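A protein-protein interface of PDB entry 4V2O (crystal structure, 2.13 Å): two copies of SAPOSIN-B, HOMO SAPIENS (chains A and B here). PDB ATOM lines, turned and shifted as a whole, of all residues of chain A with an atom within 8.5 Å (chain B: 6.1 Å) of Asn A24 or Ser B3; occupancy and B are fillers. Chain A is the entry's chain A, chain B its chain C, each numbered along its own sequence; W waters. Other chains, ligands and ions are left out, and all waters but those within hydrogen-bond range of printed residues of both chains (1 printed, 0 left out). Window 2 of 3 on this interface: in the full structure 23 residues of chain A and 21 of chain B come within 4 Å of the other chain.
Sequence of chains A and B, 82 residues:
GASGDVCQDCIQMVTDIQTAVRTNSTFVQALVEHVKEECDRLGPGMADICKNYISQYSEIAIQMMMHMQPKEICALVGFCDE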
ATOM      1  N   ASP A  16       6.545  28.115 -29.929  1.00  0.00           N
ATOM      2  CA  ASP A  16       7.198  27.350 -28.869  1.00  0.00           C
ATOM      3  C   ASP A  16       8.187  28.180 -28.046  1.00  0.00           C
ATOM      4  O   ASP A  16       8.324  27.923 -26.852  1.00  0.00           O
ATOM      5  CB  ASP A  16       7.813  26.054 -29.418  1.00  0.00           C
ATOM      6  CG  ASP A  16       6.772  25.033 -29.881  1.00  0.00           C
ATOM      7  OD1 ASP A  16       5.613  25.093 -29.405  1.00  0.00           O
ATOM      8  OD2 ASP A  16       7.126  24.151 -30.679  1.00  0.00           O
ATOM      9  N   ILE A  17       8.850  29.192 -28.659  1.00  0.00           N
ATOM     10  CA  ILE A  17       9.756  30.117 -27.945  1.00  0.00           C
ATOM     11  C   ILE A  17       8.924  30.914 -26.939  1.00  0.00           C
ATOM     12  O   ILE A  17       9.325  31.047 -25.780  1.00  0.00           O
ATOM     13  CB  ILE A  17      10.543  31.059 -28.909  1.00  0.00           C
ATOM     14  CG1 ILE A  17      11.629  30.275 -29.675  1.00  0.00           C
ATOM     15  CG2 ILE A  17      11.160  32.277 -28.159  1.00  0.00           C
ATOM     16  CD1 ILE A  17      12.183  30.981 -30.926  1.00  0.00           C
ATOM     17  N   GLN A  18       7.753  31.416 -27.378  1.00  0.00           N
ATOM     18  CA  GLN A  18       6.856  32.198 -26.534  1.00  0.00           C
ATOM     19  C   GLN A  18       6.321  31.343 -25.388  1.00  0.00           C
ATOM     20  O   GLN A  18       6.255  31.834 -24.266  1.00  0.00           O
ATOM     21  CB  GLN A  18       5.739  32.855 -27.357  1.00  0.00           C
ATOM     22  CG  GLN A  18       6.270  33.887 -28.367  1.00  0.00           C
ATOM     23  CD  GLN A  18       5.181  34.690 -29.047  1.00  0.00           C
ATOM     24  OE1 GLN A  18       4.092  34.191 -29.347  1.00  0.00           O
ATOM     25  NE2 GLN A  18       5.479  35.947 -29.347  1.00  0.00           N
ATOM     26  N   THR A  19       6.014  30.045 -25.647  1.00  0.00           N
ATOM     27  CA  THR A  19       5.566  29.096 -24.608  1.00  0.00           C
ATOM     28  C   THR A  19       6.714  28.850 -23.600  1.00  0.00           C
ATOM     29  O   THR A  19       6.462  28.807 -22.396  1.00  0.00           O
ATOM     30  CB  THR A  19       5.019  27.797 -25.241  1.00  0.00           C
ATOM     31  OG1 THR A  19       3.979  28.121 -26.172  1.00  0.00           O
ATOM     32  CG2 THR A  19       4.511  26.788 -24.202  1.00  0.00           C
ATOM     33  N   ALA A  20       7.957  28.702 -24.097  1.00  0.00           N
ATOM     34  CA  ALA A  20       9.170  28.505 -23.291  1.00  0.00           C
ATOM     35  C   ALA A  20       9.418  29.705 -22.385  1.00  0.00           C
ATOM     36  O   ALA A  20       9.699  29.520 -21.211  1.00  0.00           O
ATOM     37  CB  ALA A  20      10.372  28.285 -24.192  1.00  0.00           C
ATOM     38  N   VAL A  21       9.284  30.936 -22.919  1.00  0.00           N
ATOM     39  CA  VAL A  21       9.440  32.174 -22.145  1.00  0.00           C
ATOM     40  C   VAL A  21       8.388  32.241 -21.008  1.00  0.00           C
ATOM     41  O   VAL A  21       8.760  32.551 -19.881  1.00  0.00           O
ATOM     42  CB  VAL A  21       9.428  33.444 -23.045  1.00  0.00           C
ATOM     43  CG1 VAL A  21       9.467  34.731 -22.211  1.00  0.00           C
ATOM     44  CG2 VAL A  21      10.580  33.420 -24.043  1.00  0.00           C
ATOM     45  N   ARG A  22       7.108  31.913 -21.299  1.00  0.00           N
ATOM     46  CA  ARG A  22       6.008  31.941 -20.321  1.00  0.00           C
ATOM     47  C   ARG A  22       6.049  30.827 -19.284  1.00  0.00           C
ATOM     48  O   ARG A  22       5.593  31.044 -18.161  1.00  0.00           O
ATOM     49  CB  ARG A  22       4.638  31.928 -21.022  1.00  0.00           C
ATOM     50  CG  ARG A  22       4.375  33.194 -21.822  1.00  0.00           C
ATOM     51  CD  ARG A  22       2.924  33.375 -22.188  1.00  0.00           C
ATOM     52  NE  ARG A  22       2.754  34.545 -23.044  1.00  0.00           N
ATOM     53  CZ  ARG A  22       2.544  34.491 -24.353  1.00  0.00           C
ATOM     54  NH1 ARG A  22       2.471  33.322 -24.974  1.00  0.00           N
ATOM     55  NH2 ARG A  22       2.405  35.606 -25.055  1.00  0.00           N
ATOM     56  N   THR A  23       6.553  29.631 -19.657  1.00  0.00           N
ATOM     57  CA  THR A  23       6.574  28.470 -18.748  1.00  0.00           C
ATOM     58  C   THR A  23       7.937  28.127 -18.110  1.00  0.00           C
ATOM     59  O   THR A  23       7.965  27.432 -17.103  1.00  0.00           O
ATOM     60  CB  THR A  23       5.919  27.241 -19.415  1.00  0.00           C
ATOM     61  OG1 THR A  23       6.747  26.776 -20.492  1.00  0.00           O
ATOM     62  CG2 THR A  23       4.488  27.520 -19.898  1.00  0.00           C
ATOM     63  N   ASN A  24       9.056  28.560 -18.716  1.00  0.00           N
ATOM     64  CA  ASN A  24      10.408  28.271 -18.231  1.00  0.00           C
ATOM     65  C   ASN A  24      11.065  29.582 -17.794  1.00  0.00           C
ATOM     66  O   ASN A  24      11.417  30.415 -18.634  1.00  0.00           O
ATOM     67  CB  ASN A  24      11.221  27.523 -19.310  1.00  0.00           C
ATOM     68  CG  ASN A  24      12.635  27.130 -18.938  1.00  0.00           C
ATOM     69  OD1 ASN A  24      13.272  27.718 -18.055  1.00  0.00           O
ATOM     70  ND2 ASN A  24      13.177  26.137 -19.646  1.00  0.00           N
ATOM     71  N   SER A  25      11.220  29.751 -16.466  1.00  0.00           N
ATOM     72  CA  SER A  25      11.756  30.954 -15.818  1.00  0.00           C
ATOM     73  C   SER A  25      13.249  31.220 -16.040  1.00  0.00           C
ATOM     74  O   SER A  25      13.720  32.317 -15.735  1.00  0.00           O
ATOM     75  CB  SER A  25      11.423  30.952 -14.327  1.00  0.00           C
ATOM     76  OG  SER A  25      12.110  29.915 -13.648  1.00  0.00           O
ATOM     77  N   THR A  26      13.995  30.235 -16.560  1.00  0.00           N
ATOM     78  CA  THR A  26      15.429  30.396 -16.813  1.00  0.00           C
ATOM     79  C   THR A  26      15.761  30.459 -18.313  1.00  0.00           C
ATOM     80  O   THR A  26      16.917  30.680 -18.653  1.00  0.00           O
ATOM     81  CB  THR A  26      16.254  29.336 -16.043  1.00  0.00           C
ATOM     82  OG1 THR A  26      15.849  28.026 -16.427  1.00  0.00           O
ATOM     83  CG2 THR A  26      16.153  29.495 -14.523  1.00  0.00           C
ATOM     84  N   PHE A  27      14.756  30.274 -19.199  1.00  0.00           N
ATOM     85  CA  PHE A  27      14.908  30.245 -20.664  1.00  0.00           C
ATOM     86  C   PHE A  27      15.542  31.507 -21.244  1.00  0.00           C
ATOM     87  O   PHE A  27      16.549  31.393 -21.945  1.00  0.00           O
ATOM     88  CB  PHE A  27      13.573  29.909 -21.363  1.00  0.00           C
ATOM     89  CG  PHE A  27      13.649  29.841 -22.873  1.00  0.00           C
ATOM     90  CD1 PHE A  27      14.014  28.666 -23.516  1.00  0.00           C
ATOM     91  CD2 PHE A  27      13.370  30.965 -23.655  1.00  0.00           C
ATOM     92  CE1 PHE A  27      14.091  28.610 -24.918  1.00  0.00           C
ATOM     93  CE2 PHE A  27      13.457  30.910 -25.052  1.00  0.00           C
ATOM     94  CZ  PHE A  27      13.806  29.733 -25.675  1.00  0.00           C
ATOM     95  N   VAL A  28      14.953  32.690 -20.975  1.00  0.00           N
ATOM     96  CA  VAL A  28      15.444  33.984 -21.475  1.00  0.00           C
ATOM     97  C   VAL A  28      16.888  34.248 -21.047  1.00  0.00           C
ATOM     98  O   VAL A  28      17.739  34.490 -21.907  1.00  0.00           O
ATOM     99  CB  VAL A  28      14.488  35.161 -21.134  1.00  0.00           C
ATOM    100  CG1 VAL A  28      15.130  36.514 -21.431  1.00  0.00           C
ATOM    101  CG2 VAL A  28      13.175  35.022 -21.880  1.00  0.00           C
ATOM    102  N   GLN A  29      17.155  34.153 -19.724  1.00  0.00           N
ATOM    103  CA  GLN A  29      18.467  34.330 -19.100  1.00  0.00           C
ATOM    104  C   GLN A  29      19.525  33.422 -19.738  1.00  0.00           C
ATOM    105  O   GLN A  29      20.597  33.910 -20.092  1.00  0.00           O
ATOM    106  CB  GLN A  29      18.366  34.091 -17.584  1.00  0.00           C
ATOM    107  CG  GLN A  29      19.675  34.198 -16.830  1.00  0.00           C
ATOM    108  CD  GLN A  29      19.469  34.028 -15.349  1.00  0.00           C
ATOM    109  OE1 GLN A  29      19.112  32.950 -14.861  1.00  0.00           O
ATOM    110  NE2 GLN A  29      19.719  35.086 -14.592  1.00  0.00           N
ATOM    111  N   ALA A  30      19.214  32.119 -19.908  1.00  0.00           N
ATOM    112  CA  ALA A  30      20.123  31.148 -20.514  1.00  0.00           C
ATOM    113  C   ALA A  30      20.438  31.500 -21.972  1.00  0.00           C
ATOM    114  O   ALA A  30      21.599  31.404 -22.357  1.00  0.00           O
ATOM    115  CB  ALA A  30      19.555  29.743 -20.421  1.00  0.00           C
ATOM    116  N   GLY B   1      10.661  18.822 -22.923  1.00  0.00           N
ATOM    117  CA  GLY B   1       9.921  19.984 -22.449  1.00  0.00           C
ATOM    118  C   GLY B   1       9.906  21.111 -23.453  1.00  0.00           C
ATOM    119  O   GLY B   1      10.350  20.928 -24.591  1.00  0.00           O
ATOM    120  N   ALA B   2       9.405  22.285 -23.039  1.00  0.00           N
ATOM    121  CA  ALA B   2       9.322  23.449 -23.934  1.00  0.00           C
ATOM    122  C   ALA B   2      10.647  23.824 -24.599  1.00  0.00           C
ATOM    123  O   ALA B   2      10.648  24.033 -25.805  1.00  0.00           O
ATOM    124  CB  ALA B   2       8.727  24.641 -23.208  1.00  0.00           C
ATOM    125  N   SER B   3      11.782  23.856 -23.847  1.00  0.00           N
ATOM    126  CA  SER B   3      13.117  24.160 -24.407  1.00  0.00           C
ATOM    127  C   SER B   3      13.521  23.124 -25.446  1.00  0.00           C
ATOM    128  O   SER B   3      14.092  23.493 -26.475  1.00  0.00           O
ATOM    129  CB  SER B   3      14.189  24.219 -23.324  1.00  0.00           C
ATOM    130  OG  SER B   3      13.783  25.018 -22.227  1.00  0.00           O
ATOM    131  N   GLY B   4      13.195  21.851 -25.176  1.00  0.00           N
ATOM    132  CA  GLY B   4      13.433  20.735 -26.088  1.00  0.00           C
ATOM    133  C   GLY B   4      12.633  20.874 -27.373  1.00  0.00           C
ATOM    134  O   GLY B   4      13.142  20.564 -28.448  1.00  0.00           O
ATOM    135  N   ASP B   5      11.370  21.376 -27.273  1.00  0.00           N
ATOM    136  CA  ASP B   5      10.512  21.620 -28.442  1.00  0.00           C
ATOM    137  C   ASP B   5      11.122  22.688 -29.354  1.00  0.00           C
ATOM    138  O   ASP B   5      11.146  22.475 -30.556  1.00  0.00           O
ATOM    139  CB  ASP B   5       9.080  22.008 -28.037  1.00  0.00           C
ATOM    140  CG  ASP B   5       8.304  20.890 -27.360  1.00  0.00           C
ATOM    141  OD1 ASP B   5       8.663  19.700 -27.565  1.00  0.00           O
ATOM    142  OD2 ASP B   5       7.349  21.198 -26.621  1.00  0.00           O
ATOM    143  N   VAL B   6      11.640  23.803 -28.783  1.00  0.00           N
ATOM    144  CA  VAL B   6      12.291  24.896 -29.525  1.00  0.00           C
ATOM    145  C   VAL B   6      13.495  24.384 -30.321  1.00  0.00           C
ATOM    146  O   VAL B   6      13.669  24.758 -31.484  1.00  0.00           O
ATOM    147  CB  VAL B   6      12.671  26.076 -28.592  1.00  0.00           C
ATOM    148  CG1 VAL B   6      13.582  27.093 -29.290  1.00  0.00           C
ATOM    149  CG2 VAL B   6      11.424  26.742 -28.022  1.00  0.00           C
ATOM    150  N   CYS B   7      14.315  23.526 -29.695  1.00  0.00           N
ATOM    151  CA  CYS B   7      15.487  22.944 -30.339  1.00  0.00           C
ATOM    152  C   CYS B   7      15.118  22.174 -31.609  1.00  0.00           C
ATOM    153  O   CYS B   7      15.699  22.431 -32.667  1.00  0.00           O
ATOM    154  CB  CYS B   7      16.271  22.077 -29.361  1.00  0.00           C
ATOM    155  SG  CYS B   7      17.632  21.172 -30.125  1.00  0.00           S
ATOM    156  N   GLN B   8      14.152  21.244 -31.496  1.00  0.00           N
ATOM    157  CA  GLN B   8      13.684  20.426 -32.617  1.00  0.00           C
ATOM    158  C   GLN B   8      13.049  21.292 -33.710  1.00  0.00           C
ATOM    159  O   GLN B   8      13.245  21.036 -34.903  1.00  0.00           O
ATOM    160  CB  GLN B   8      12.697  19.339 -32.140  1.00  0.00           C
ATOM    161  CG  GLN B   8      13.312  18.188 -31.326  1.00  0.00           C
ATOM    162  CD  GLN B   8      14.420  17.386 -31.993  1.00  0.00           C
ATOM    163  OE1 GLN B   8      14.602  17.361 -33.222  1.00  0.00           O
ATOM    164  NE2 GLN B   8      15.169  16.665 -31.175  1.00  0.00           N
ATOM    165  N   PHE B  79      19.266  27.994 -29.441  1.00  0.00           N
ATOM    166  CA  PHE B  79      17.986  27.276 -29.416  1.00  0.00           C
ATOM    167  C   PHE B  79      18.142  25.789 -29.103  1.00  0.00           C
ATOM    168  O   PHE B  79      17.176  25.164 -28.671  1.00  0.00           O
ATOM    169  CB  PHE B  79      17.148  27.540 -30.679  1.00  0.00           C
ATOM    170  CG  PHE B  79      16.748  28.985 -30.884  1.00  0.00           C
ATOM    171  CD1 PHE B  79      16.330  29.769 -29.815  1.00  0.00           C
ATOM    172  CD2 PHE B  79      16.745  29.550 -32.154  1.00  0.00           C
ATOM    173  CE1 PHE B  79      15.950  31.102 -30.010  1.00  0.00           C
ATOM    174  CE2 PHE B  79      16.361  30.882 -32.347  1.00  0.00           C
ATOM    175  CZ  PHE B  79      15.965  31.647 -31.273  1.00  0.00           C
HETATM  176  O   HOH W   1       8.091  25.424 -26.239  1.00  0.00           O
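Water W1 lies within hydrogen-bond range of the backbone carbonyl oxygen of Asp A16 and the backbone carbonyl oxygen of Ala B2.
The side-chain amide nitrogen (ND2) of Asn A24 is in hydrogen-bond range of the side-chain hydroxyl (OG) of Ser B3 (2.9 Å).
OD2 of Asp A16 touches CB of Asp B5, 3.9 Å away.
CG2 of Val B6 touches O of Asp A16, 3.5 Å away.
CG2 of Val B6 touches N of Ile A17, at 3.6 Å.
Ile A17 touches Phe B79.
Ala A20 touches Ala B2 (CA to CB, 3.9 Å).
Ala B2 touches Thr A23 (CB to OG1, 3.98 Å).
Ser B3 touches Phe A27 (OG to CD1, 3.9 Å).
The backbone carbonyl oxygen of Phe B79 sits close to the backbone NH of Cys B7 (3.5 Å).
OG1 of Thr A23 is in hydrogen-bond range of O of Thr A19.
N of Thr A26 is in hydrogen-bond range of OD1 of Asn A24.
The side-chain amide oxygen (OD1) of Asn A24 sits at hydrogen-bond distance from the backbone NH (N) of Phe A27.
Of the 9 printed residues of chain B, 5 touch a printed residue of chain A.
Printed residues of chain B that touch a printed residue of chain A: Ala B2, Ser B3, Asp B5, Val B6 and Phe B79.
Along chain A the printed residues that touch a printed residue of chain B span positions 16 to 27.
Among the printed residues, 8 pairs touch across the chains.
No position is printed for both chains.
Of the printed residues of chain B, Ile A17 touches Val B6 and Phe B79.
Of the printed residues of chain B, Ala A20 touches Ala B2 (3.9 Å).
Of the printed residues of chain B, Asn A24 touches Ser B3.
Ser B3 touches just these residues of chain A: Asn A24 (2.9 Å) and Phe A27 (3.9 Å).
Gly B4 touches none of the printed residues of chain A.
The nearest residue of chain A that does not touch Ser B3 is Ala A20 (4.7 Å).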
